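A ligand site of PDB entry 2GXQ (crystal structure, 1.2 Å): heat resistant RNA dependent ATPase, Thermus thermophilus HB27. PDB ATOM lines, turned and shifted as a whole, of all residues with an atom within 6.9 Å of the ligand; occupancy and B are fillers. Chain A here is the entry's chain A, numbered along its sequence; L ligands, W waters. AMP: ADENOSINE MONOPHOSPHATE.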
ATOM      1  N   PHE A   3     -17.796  -0.259  -1.450  1.00  0.00           N
ATOM      2  CA  PHE A   3     -17.182   0.839  -2.159  1.00  0.00           C
ATOM      3  C   PHE A   3     -18.144   1.927  -2.488  1.00  0.00           C
ATOM      4  O   PHE A   3     -17.789   3.084  -2.388  1.00  0.00           O
ATOM      5  CB  PHE A   3     -16.467   0.369  -3.437  1.00  0.00           C
ATOM      6  CG  PHE A   3     -15.152  -0.308  -3.162  1.00  0.00           C
ATOM      7  CD1 PHE A   3     -14.123   0.382  -2.544  1.00  0.00           C
ATOM      8  CD2 PHE A   3     -14.947  -1.603  -3.500  1.00  0.00           C
ATOM      9  CE1 PHE A   3     -12.936  -0.273  -2.302  1.00  0.00           C
ATOM     10  CE2 PHE A   3     -13.757  -2.243  -3.257  1.00  0.00           C
ATOM     11  CZ  PHE A   3     -12.759  -1.556  -2.646  1.00  0.00           C
ATOM     12  N   LEU A  16     -14.800  -0.849 -10.603  1.00  0.00           N
ATOM     13  CA  LEU A  16     -14.719  -1.782  -9.500  1.00  0.00           C
ATOM     14  C   LEU A  16     -15.736  -2.923  -9.653  1.00  0.00           C
ATOM     15  O   LEU A  16     -15.385  -4.079  -9.600  1.00  0.00           O
ATOM     16  CB  LEU A  16     -14.930  -1.065  -8.187  1.00  0.00           C
ATOM     17  CG  LEU A  16     -13.797  -0.143  -7.716  1.00  0.00           C
ATOM     18  CD1 LEU A  16     -14.279   0.690  -6.566  1.00  0.00           C
ATOM     19  CD2 LEU A  16     -12.568  -0.938  -7.337  1.00  0.00           C
ATOM     20  N   ARG A  19     -14.901  -5.682 -12.070  1.00  0.00           N
ATOM     21  CA  ARG A  19     -13.947  -6.657 -11.639  1.00  0.00           C
ATOM     22  C   ARG A  19     -14.407  -7.402 -10.409  1.00  0.00           C
ATOM     23  O   ARG A  19     -13.651  -8.151  -9.816  1.00  0.00           O
ATOM     24  CB  ARG A  19     -12.623  -6.000 -11.395  1.00  0.00           C
ATOM     25  CG  ARG A  19     -12.090  -5.493 -12.721  1.00  0.00           C
ATOM     26  CD  ARG A  19     -10.634  -5.543 -12.725  1.00  0.00           C
ATOM     27  NE  ARG A  19     -10.203  -4.578 -11.742  1.00  0.00           N
ATOM     28  CZ  ARG A  19      -8.999  -4.552 -11.194  1.00  0.00           C
ATOM     29  NH1 ARG A  19      -8.059  -5.407 -11.548  1.00  0.00           N
ATOM     30  NH2 ARG A  19      -8.760  -3.617 -10.314  1.00  0.00           N
ATOM     31  N   GLY A  20     -15.650  -7.203 -10.006  1.00  0.00           N
ATOM     32  CA  GLY A  20     -16.172  -7.905  -8.840  1.00  0.00           C
ATOM     33  C   GLY A  20     -15.648  -7.386  -7.527  1.00  0.00           C
ATOM     34  O   GLY A  20     -15.659  -8.121  -6.533  1.00  0.00           O
ATOM     35  N   LEU A  21     -15.184  -6.143  -7.502  1.00  0.00           N
ATOM     36  CA  LEU A  21     -14.645  -5.542  -6.303  1.00  0.00           C
ATOM     37  C   LEU A  21     -15.739  -4.702  -5.693  1.00  0.00           C
ATOM     38  O   LEU A  21     -16.232  -3.781  -6.272  1.00  0.00           O
ATOM     39  CB  LEU A  21     -13.457  -4.666  -6.655  1.00  0.00           C
ATOM     40  CG  LEU A  21     -12.298  -5.424  -7.229  1.00  0.00           C
ATOM     41  CD1 LEU A  21     -11.311  -4.437  -7.930  1.00  0.00           C
ATOM     42  CD2 LEU A  21     -11.649  -6.311  -6.202  1.00  0.00           C
ATOM     43  N   THR A  22     -16.150  -5.115  -4.507  1.00  0.00           N
ATOM     44  CA  THR A  22     -17.285  -4.501  -3.829  1.00  0.00           C
ATOM     45  C   THR A  22     -17.039  -3.968  -2.433  1.00  0.00           C
ATOM     46  O   THR A  22     -17.714  -3.031  -2.013  1.00  0.00           O
ATOM     47  CB  THR A  22     -18.444  -5.538  -3.685  1.00  0.00           C
ATOM     48  OG1 THR A  22     -18.057  -6.584  -2.805  1.00  0.00           O
ATOM     49  CG2 THR A  22     -18.767  -6.125  -5.015  1.00  0.00           C
ATOM     50  N   THR A  23     -16.123  -4.599  -1.710  1.00  0.00           N
ATOM     51  CA  THR A  23     -16.048  -4.362  -0.284  1.00  0.00           C
ATOM     52  C   THR A  23     -14.609  -4.074   0.095  1.00  0.00           C
ATOM     53  O   THR A  23     -13.749  -4.929  -0.101  1.00  0.00           O
ATOM     54  CB  THR A  23     -16.526  -5.619   0.412  1.00  0.00           C
ATOM     55  OG1 THR A  23     -17.847  -5.930  -0.073  1.00  0.00           O
ATOM     56  CG2 THR A  23     -16.569  -5.424   1.923  1.00  0.00           C
ATOM     57  N   PRO A  24     -14.340  -2.890   0.577  1.00  0.00           N
ATOM     58  CA  PRO A  24     -12.985  -2.593   0.922  1.00  0.00           C
ATOM     59  C   PRO A  24     -12.380  -3.508   1.936  1.00  0.00           C
ATOM     60  O   PRO A  24     -13.057  -3.947   2.873  1.00  0.00           O
ATOM     61  CB  PRO A  24     -13.072  -1.168   1.456  1.00  0.00           C
ATOM     62  CG  PRO A  24     -14.424  -0.794   1.529  1.00  0.00           C
ATOM     63  CD  PRO A  24     -15.216  -1.722   0.714  1.00  0.00           C
ATOM     64  N   THR A  25     -11.111  -3.815   1.779  1.00  0.00           N
ATOM     65  CA  THR A  25     -10.362  -4.522   2.762  1.00  0.00           C
ATOM     66  C   THR A  25     -10.107  -3.588   3.950  1.00  0.00           C
ATOM     67  O   THR A  25     -10.353  -2.404   3.854  1.00  0.00           O
ATOM     68  CB  THR A  25      -9.009  -4.954   2.193  1.00  0.00           C
ATOM     69  OG1 THR A  25      -8.277  -3.770   1.911  1.00  0.00           O
ATOM     70  CG2 THR A  25      -9.145  -5.804   0.935  1.00  0.00           C
ATOM     71  N   ILE A  27      -7.492  -2.118   5.284  1.00  0.00           N
ATOM     72  CA  ILE A  27      -6.706  -0.931   5.076  1.00  0.00           C
ATOM     73  C   ILE A  27      -7.419   0.040   4.164  1.00  0.00           C
ATOM     74  O   ILE A  27      -7.324   1.243   4.346  1.00  0.00           O
ATOM     75  CB  ILE A  27      -5.289  -1.220   4.613  1.00  0.00           C
ATOM     76  CG1 ILE A  27      -4.435   0.011   4.783  1.00  0.00           C
ATOM     77  CG2 ILE A  27      -5.250  -1.733   3.175  1.00  0.00           C
ATOM     78  CD1 ILE A  27      -2.953  -0.215   4.619  1.00  0.00           C
ATOM     79  N   GLN A  28      -8.184  -0.477   3.197  1.00  0.00           N
ATOM     80  CA  GLN A  28      -8.964   0.409   2.342  1.00  0.00           C
ATOM     81  C   GLN A  28     -10.069   1.109   3.102  1.00  0.00           C
ATOM     82  O   GLN A  28     -10.309   2.295   2.929  1.00  0.00           O
ATOM     83  CB  GLN A  28      -9.531  -0.397   1.191  1.00  0.00           C
ATOM     84  CG  GLN A  28      -8.491  -0.964   0.268  1.00  0.00           C
ATOM     85  CD  GLN A  28      -8.972  -2.054  -0.592  1.00  0.00           C
ATOM     86  OE1 GLN A  28     -10.150  -2.438  -0.577  1.00  0.00           O
ATOM     87  NE2 GLN A  28      -8.064  -2.613  -1.384  1.00  0.00           N
ATOM     88  N   ARG A  46       1.462  -4.930   4.090  1.00  0.00           N
ATOM     89  CA  ARG A  46       2.157  -5.666   3.049  1.00  0.00           C
ATOM     90  C   ARG A  46       1.172  -6.100   1.985  1.00  0.00           C
ATOM     91  O   ARG A  46      -0.046  -6.054   2.169  1.00  0.00           O
ATOM     92  CB  ARG A  46       2.786  -6.926   3.662  1.00  0.00           C
ATOM     93  CG  ARG A  46       3.848  -6.697   4.701  1.00  0.00           C
ATOM     94  CD  ARG A  46       4.407  -8.034   5.179  1.00  0.00           C
ATOM     95  NE  ARG A  46       5.260  -7.798   6.343  1.00  0.00           N
ATOM     96  CZ  ARG A  46       6.506  -7.358   6.257  1.00  0.00           C
ATOM     97  NH1 ARG A  46       7.199  -7.137   7.374  1.00  0.00           N
ATOM     98  NH2 ARG A  46       7.065  -7.127   5.072  1.00  0.00           N
ATOM     99  N   THR A  47       1.687  -6.523   0.851  1.00  0.00           N
ATOM    100  CA  THR A  47       0.872  -7.114  -0.201  1.00  0.00           C
ATOM    101  C   THR A  47      -0.009  -8.178   0.374  1.00  0.00           C
ATOM    102  O   THR A  47       0.409  -8.978   1.236  1.00  0.00           O
ATOM    103  CB  THR A  47       1.689  -7.756  -1.383  1.00  0.00           C
ATOM    104  OG1 THR A  47       0.783  -8.096  -2.435  1.00  0.00           O
ATOM    105  CG2 THR A  47       2.394  -9.063  -0.983  1.00  0.00           C
ATOM    106  N   GLY A  48      -1.236  -8.231  -0.137  1.00  0.00           N
ATOM    107  CA  GLY A  48      -2.273  -9.122   0.338  1.00  0.00           C
ATOM    108  C   GLY A  48      -3.362  -8.419   1.114  1.00  0.00           C
ATOM    109  O   GLY A  48      -4.419  -8.967   1.346  1.00  0.00           O
ATOM    110  N   THR A  49      -3.063  -7.203   1.571  1.00  0.00           N
ATOM    111  CA  THR A  49      -4.002  -6.402   2.331  1.00  0.00           C
ATOM    112  C   THR A  49      -4.917  -5.552   1.505  1.00  0.00           C
ATOM    113  O   THR A  49      -5.822  -4.969   2.029  1.00  0.00           O
ATOM    114  CB  THR A  49      -3.242  -5.525   3.282  1.00  0.00           C
ATOM    115  OG1 THR A  49      -2.358  -4.649   2.565  1.00  0.00           O
ATOM    116  CG2 THR A  49      -2.559  -6.284   4.376  1.00  0.00           C
ATOM    117  N   GLY A  50      -4.603  -5.391   0.217  1.00  0.00           N
ATOM    118  CA  GLY A  50      -5.304  -4.426  -0.610  1.00  0.00           C
ATOM    119  C   GLY A  50      -4.717  -3.047  -0.530  1.00  0.00           C
ATOM    120  O   GLY A  50      -5.395  -2.066  -0.809  1.00  0.00           O
ATOM    121  N   LYS A  51      -3.442  -2.945  -0.209  1.00  0.00           N
ATOM    122  CA  LYS A  51      -2.864  -1.637  -0.115  1.00  0.00           C
ATOM    123  C   LYS A  51      -2.849  -0.896  -1.432  1.00  0.00           C
ATOM    124  O   LYS A  51      -2.957   0.318  -1.429  1.00  0.00           O
ATOM    125  CB  LYS A  51      -1.473  -1.714   0.451  1.00  0.00           C
ATOM    126  CG  LYS A  51      -0.525  -2.568  -0.279  1.00  0.00           C
ATOM    127  CD  LYS A  51       0.898  -2.320   0.094  1.00  0.00           C
ATOM    128  CE  LYS A  51       1.811  -3.270  -0.602  1.00  0.00           C
ATOM    129  NZ  LYS A  51       2.980  -2.507  -0.913  1.00  0.00           N
ATOM    130  N   THR A  52      -2.767  -1.579  -2.565  1.00  0.00           N
ATOM    131  CA  THR A  52      -2.702  -0.877  -3.839  1.00  0.00           C
ATOM    132  C   THR A  52      -3.907  -0.034  -4.066  1.00  0.00           C
ATOM    133  O   THR A  52      -3.800   1.131  -4.397  1.00  0.00           O
ATOM    134  CB  THR A  52      -2.503  -1.821  -4.983  1.00  0.00           C
ATOM    135  OG1 THR A  52      -1.346  -2.637  -4.694  1.00  0.00           O
ATOM    136  CG2 THR A  52      -2.302  -1.040  -6.272  1.00  0.00           C
ATOM    137  N   LEU A  53      -5.094  -0.601  -3.898  1.00  0.00           N
ATOM    138  CA  LEU A  53      -6.297   0.204  -4.099  1.00  0.00           C
ATOM    139  C   LEU A  53      -6.460   1.277  -3.068  1.00  0.00           C
ATOM    140  O   LEU A  53      -7.138   2.265  -3.323  1.00  0.00           O
ATOM    141  CB  LEU A  53      -7.551  -0.643  -4.191  1.00  0.00           C
ATOM    142  CG  LEU A  53      -7.602  -1.603  -5.364  1.00  0.00           C
ATOM    143  CD1 LEU A  53      -8.950  -2.291  -5.460  1.00  0.00           C
ATOM    144  CD2 LEU A  53      -7.247  -0.919  -6.635  1.00  0.00           C
ATOM    145  N   ALA A  54      -5.885   1.120  -1.877  1.00  0.00           N
ATOM    146  CA  ALA A  54      -5.930   2.147  -0.896  1.00  0.00           C
ATOM    147  C   ALA A  54      -5.295   3.435  -1.397  1.00  0.00           C
ATOM    148  O   ALA A  54      -5.671   4.480  -0.944  1.00  0.00           O
ATOM    149  CB  ALA A  54      -5.284   1.687   0.405  1.00  0.00           C
ATOM    150  N   PHE A  55      -4.317   3.364  -2.307  1.00  0.00           N
ATOM    151  CA  PHE A  55      -3.805   4.562  -2.912  1.00  0.00           C
ATOM    152  C   PHE A  55      -4.295   4.758  -4.347  1.00  0.00           C
ATOM    153  O   PHE A  55      -4.388   5.917  -4.778  1.00  0.00           O
ATOM    154  CB  PHE A  55      -2.296   4.679  -2.825  1.00  0.00           C
ATOM    155  CG  PHE A  55      -1.502   3.634  -3.544  1.00  0.00           C
ATOM    156  CD1 PHE A  55      -0.910   2.622  -2.880  1.00  0.00           C
ATOM    157  CD2 PHE A  55      -1.273   3.755  -4.904  1.00  0.00           C
ATOM    158  CE1 PHE A  55      -0.098   1.735  -3.509  1.00  0.00           C
ATOM    159  CE2 PHE A  55      -0.483   2.864  -5.536  1.00  0.00           C
ATOM    160  CZ  PHE A  55       0.119   1.856  -4.844  1.00  0.00           C
ATOM    161  N   LEU A  84       6.721  -4.476  -9.454  1.00  0.00           N
ATOM    162  CA  LEU A  84       5.661  -3.804  -8.726  1.00  0.00           C
ATOM    163  C   LEU A  84       5.205  -2.587  -9.496  1.00  0.00           C
ATOM    164  O   LEU A  84       4.035  -2.284  -9.472  1.00  0.00           O
ATOM    165  CB  LEU A  84       6.118  -3.436  -7.313  1.00  0.00           C
ATOM    166  CG  LEU A  84       4.984  -2.897  -6.372  1.00  0.00           C
ATOM    167  CD1 LEU A  84       3.850  -3.881  -6.233  1.00  0.00           C
ATOM    168  CD2 LEU A  84       5.478  -2.512  -4.981  1.00  0.00           C
ATOM    169  N   GLN A  87       2.728  -3.925 -11.959  1.00  0.00           N
ATOM    170  CA  GLN A  87       1.529  -4.418 -11.287  1.00  0.00           C
ATOM    171  C   GLN A  87       0.684  -3.226 -10.820  1.00  0.00           C
ATOM    172  O   GLN A  87      -0.523  -3.194 -11.025  1.00  0.00           O
ATOM    173  CB  GLN A  87       1.895  -5.267 -10.070  1.00  0.00           C
ATOM    174  CG  GLN A  87       2.490  -6.672 -10.321  1.00  0.00           C
ATOM    175  CD  GLN A  87       2.981  -7.372  -9.048  1.00  0.00           C
ATOM    176  OE1 GLN A  87       3.275  -6.739  -8.003  1.00  0.00           O
ATOM    177  NE2 GLN A  87       3.128  -8.696  -9.146  1.00  0.00           N
ATOM    178  N   GLU A  91      -3.084  -2.011 -12.063  1.00  0.00           N
ATOM    179  CA  GLU A  91      -4.213  -1.852 -11.160  1.00  0.00           C
ATOM    180  C   GLU A  91      -4.786  -0.466 -11.229  1.00  0.00           C
ATOM    181  O   GLU A  91      -6.000  -0.289 -11.277  1.00  0.00           O
ATOM    182  CB  GLU A  91      -3.794  -2.229  -9.761  1.00  0.00           C
ATOM    183  CG  GLU A  91      -4.975  -2.414  -8.832  1.00  0.00           C
ATOM    184  CD  GLU A  91      -5.832  -3.639  -9.130  1.00  0.00           C
ATOM    185  OE1 GLU A  91      -5.613  -4.327 -10.156  1.00  0.00           O
ATOM    186  OE2 GLU A  91      -6.755  -3.924  -8.345  1.00  0.00           O
HETATM  187  P   AMP L   1      -2.387  -5.709  -2.660  1.00  0.00           P
HETATM  188  O1P AMP L   1      -2.721  -4.340  -3.076  1.00  0.00           O
HETATM  189  O2P AMP L   1      -1.182  -6.261  -3.384  1.00  0.00           O
HETATM  190  O3P AMP L   1      -2.304  -5.927  -1.189  1.00  0.00           O
HETATM  191  O5' AMP L   1      -3.627  -6.575  -3.194  1.00  0.00           O
HETATM  192  C5' AMP L   1      -3.719  -7.961  -2.950  1.00  0.00           C
HETATM  193  C4' AMP L   1      -4.875  -8.554  -3.666  1.00  0.00           C
HETATM  194  O4' AMP L   1      -6.142  -8.103  -3.214  1.00  0.00           O
HETATM  195  C3' AMP L   1      -4.879  -8.305  -5.146  1.00  0.00           C
HETATM  196  O3' AMP L   1      -5.124  -9.603  -5.739  1.00  0.00           O
HETATM  197  C2' AMP L   1      -6.071  -7.415  -5.361  1.00  0.00           C
HETATM  198  O2' AMP L   1      -6.741  -7.606  -6.578  1.00  0.00           O
HETATM  199  C1' AMP L   1      -7.020  -7.885  -4.321  1.00  0.00           C
HETATM  200  N9  AMP L   1      -7.954  -6.896  -3.795  1.00  0.00           N
HETATM  201  C8  AMP L   1      -7.621  -5.654  -3.417  1.00  0.00           C
HETATM  202  N7  AMP L   1      -8.655  -5.035  -2.895  1.00  0.00           N
HETATM  203  C5  AMP L   1      -9.673  -5.886  -2.940  1.00  0.00           C
HETATM  204  C6  AMP L   1     -11.023  -5.830  -2.490  1.00  0.00           C
HETATM  205  N6  AMP L   1     -11.435  -4.748  -1.907  1.00  0.00           N
HETATM  206  N1  AMP L   1     -11.811  -6.890  -2.706  1.00  0.00           N
HETATM  207  C2  AMP L   1     -11.307  -7.988  -3.275  1.00  0.00           C
HETATM  208  N3  AMP L   1     -10.058  -8.116  -3.662  1.00  0.00           N
HETATM  209  C4  AMP L   1      -9.225  -7.089  -3.502  1.00  0.00           C
HETATM  210  O   HOH W   1     -14.621  -6.860  -2.837  1.00  0.00           O
HETATM  211  O   HOH W   2     -13.526  -9.457  -5.487  1.00  0.00           O
HETATM  212  O   HOH W   3       1.206  -4.951  -3.846  1.00  0.00           O
HETATM  213  O   HOH W   4      -5.144  -4.386  -6.281  1.00  0.00           O
HETATM  214  O   HOH W   5      -1.104  -7.456  -5.622  1.00  0.00           O
HETATM  215  O   HOH W   6      -5.201  -3.535  -3.783  1.00  0.00           O
HETATM  216  O   HOH W   7      -7.881  -8.931  -0.846  1.00  0.00           O
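OG1 of Thr 49 is in hydrogen-bond range of O of Arg 46 (2.7 Å).
The backbone NH (N) of Phe 3 sits at hydrogen-bond distance from the backbone carbonyl oxygen (O) of Thr 22 (2.8 Å).
The side-chain hydroxyl (OG1) of Thr 49 is in hydrogen-bond range of the backbone NH (N) of Lys 51.
OE1 of Gln 28 is in hydrogen-bond range of N of Thr 25, at 2.9 Å.
The side-chain hydroxyl of Thr 25 sits at hydrogen-bond distance from the backbone carbonyl oxygen of Thr 49 (2.7 Å).
The backbone carbonyl oxygen of Gly 50 is in hydrogen-bond range of the side-chain amide nitrogen of Gln 28 (2.8 Å).
O of Leu 16 is in hydrogen-bond range of N of Leu 21.
The side-chain hydroxyl (OG1) of Thr 23 sits at hydrogen-bond distance from the side-chain hydroxyl (OG1) of Thr 22 (2.8 Å).
Water W6 lies within hydrogen-bond range of an oxygen (O1P) of the ligand (2.7 Å), the backbone NH (N) of Leu 53 (2.9 Å), the backbone carbonyl oxygen (O) of Gly 50 (3.3 Å) and the backbone NH (N) of Thr 52 (3.4 Å).
Water W3 lies within hydrogen-bond range of an oxygen (O2P) of the ligand (2.8 Å) and the side-chain hydroxyl of Thr 47 (3.5 Å).
Water W1 lies within hydrogen-bond range of a nitrogen (N1) of the ligand (2.8 Å), the backbone NH (N) of Thr 22 (2.9 Å) and the backbone NH (N) of Thr 23 (2.9 Å).
Residues that only touch the ligand: Phe 3 (3.5 Å), Leu 21 (3.4 Å), Pro 24 (3.9 Å), Thr 25 (3.8 Å) and Leu 53 (3.8 Å).
The side-chain hydroxyl (OG1) of Thr 47 is in hydrogen-bond range of an oxygen (O2P) of the ligand (2.9 Å).
A nitrogen (N7) of the ligand sits at hydrogen-bond distance from the side-chain amide nitrogen (NE2) of Gln 28 (2.9 Å).
O3P of the ligand sits at hydrogen-bond distance from N of Gly 48.
N of Gly 50 is in hydrogen-bond range of O3P of the ligand (2.7 Å).
OG1 of Thr 52 sits at hydrogen-bond distance from O1P of the ligand (2.7 Å).
The backbone NH (N) of Thr 49 lies within hydrogen-bond range of an oxygen (O3P) of the ligand.
N6 of the ligand lies within hydrogen-bond range of O of Thr 23 (2.9 Å).
N of Lys 51 lies within hydrogen-bond range of O1P of the ligand (3.3 Å).
The backbone NH (N) of Thr 52 sits at hydrogen-bond distance from an oxygen (O1P) of the ligand, at 2.8 Å.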
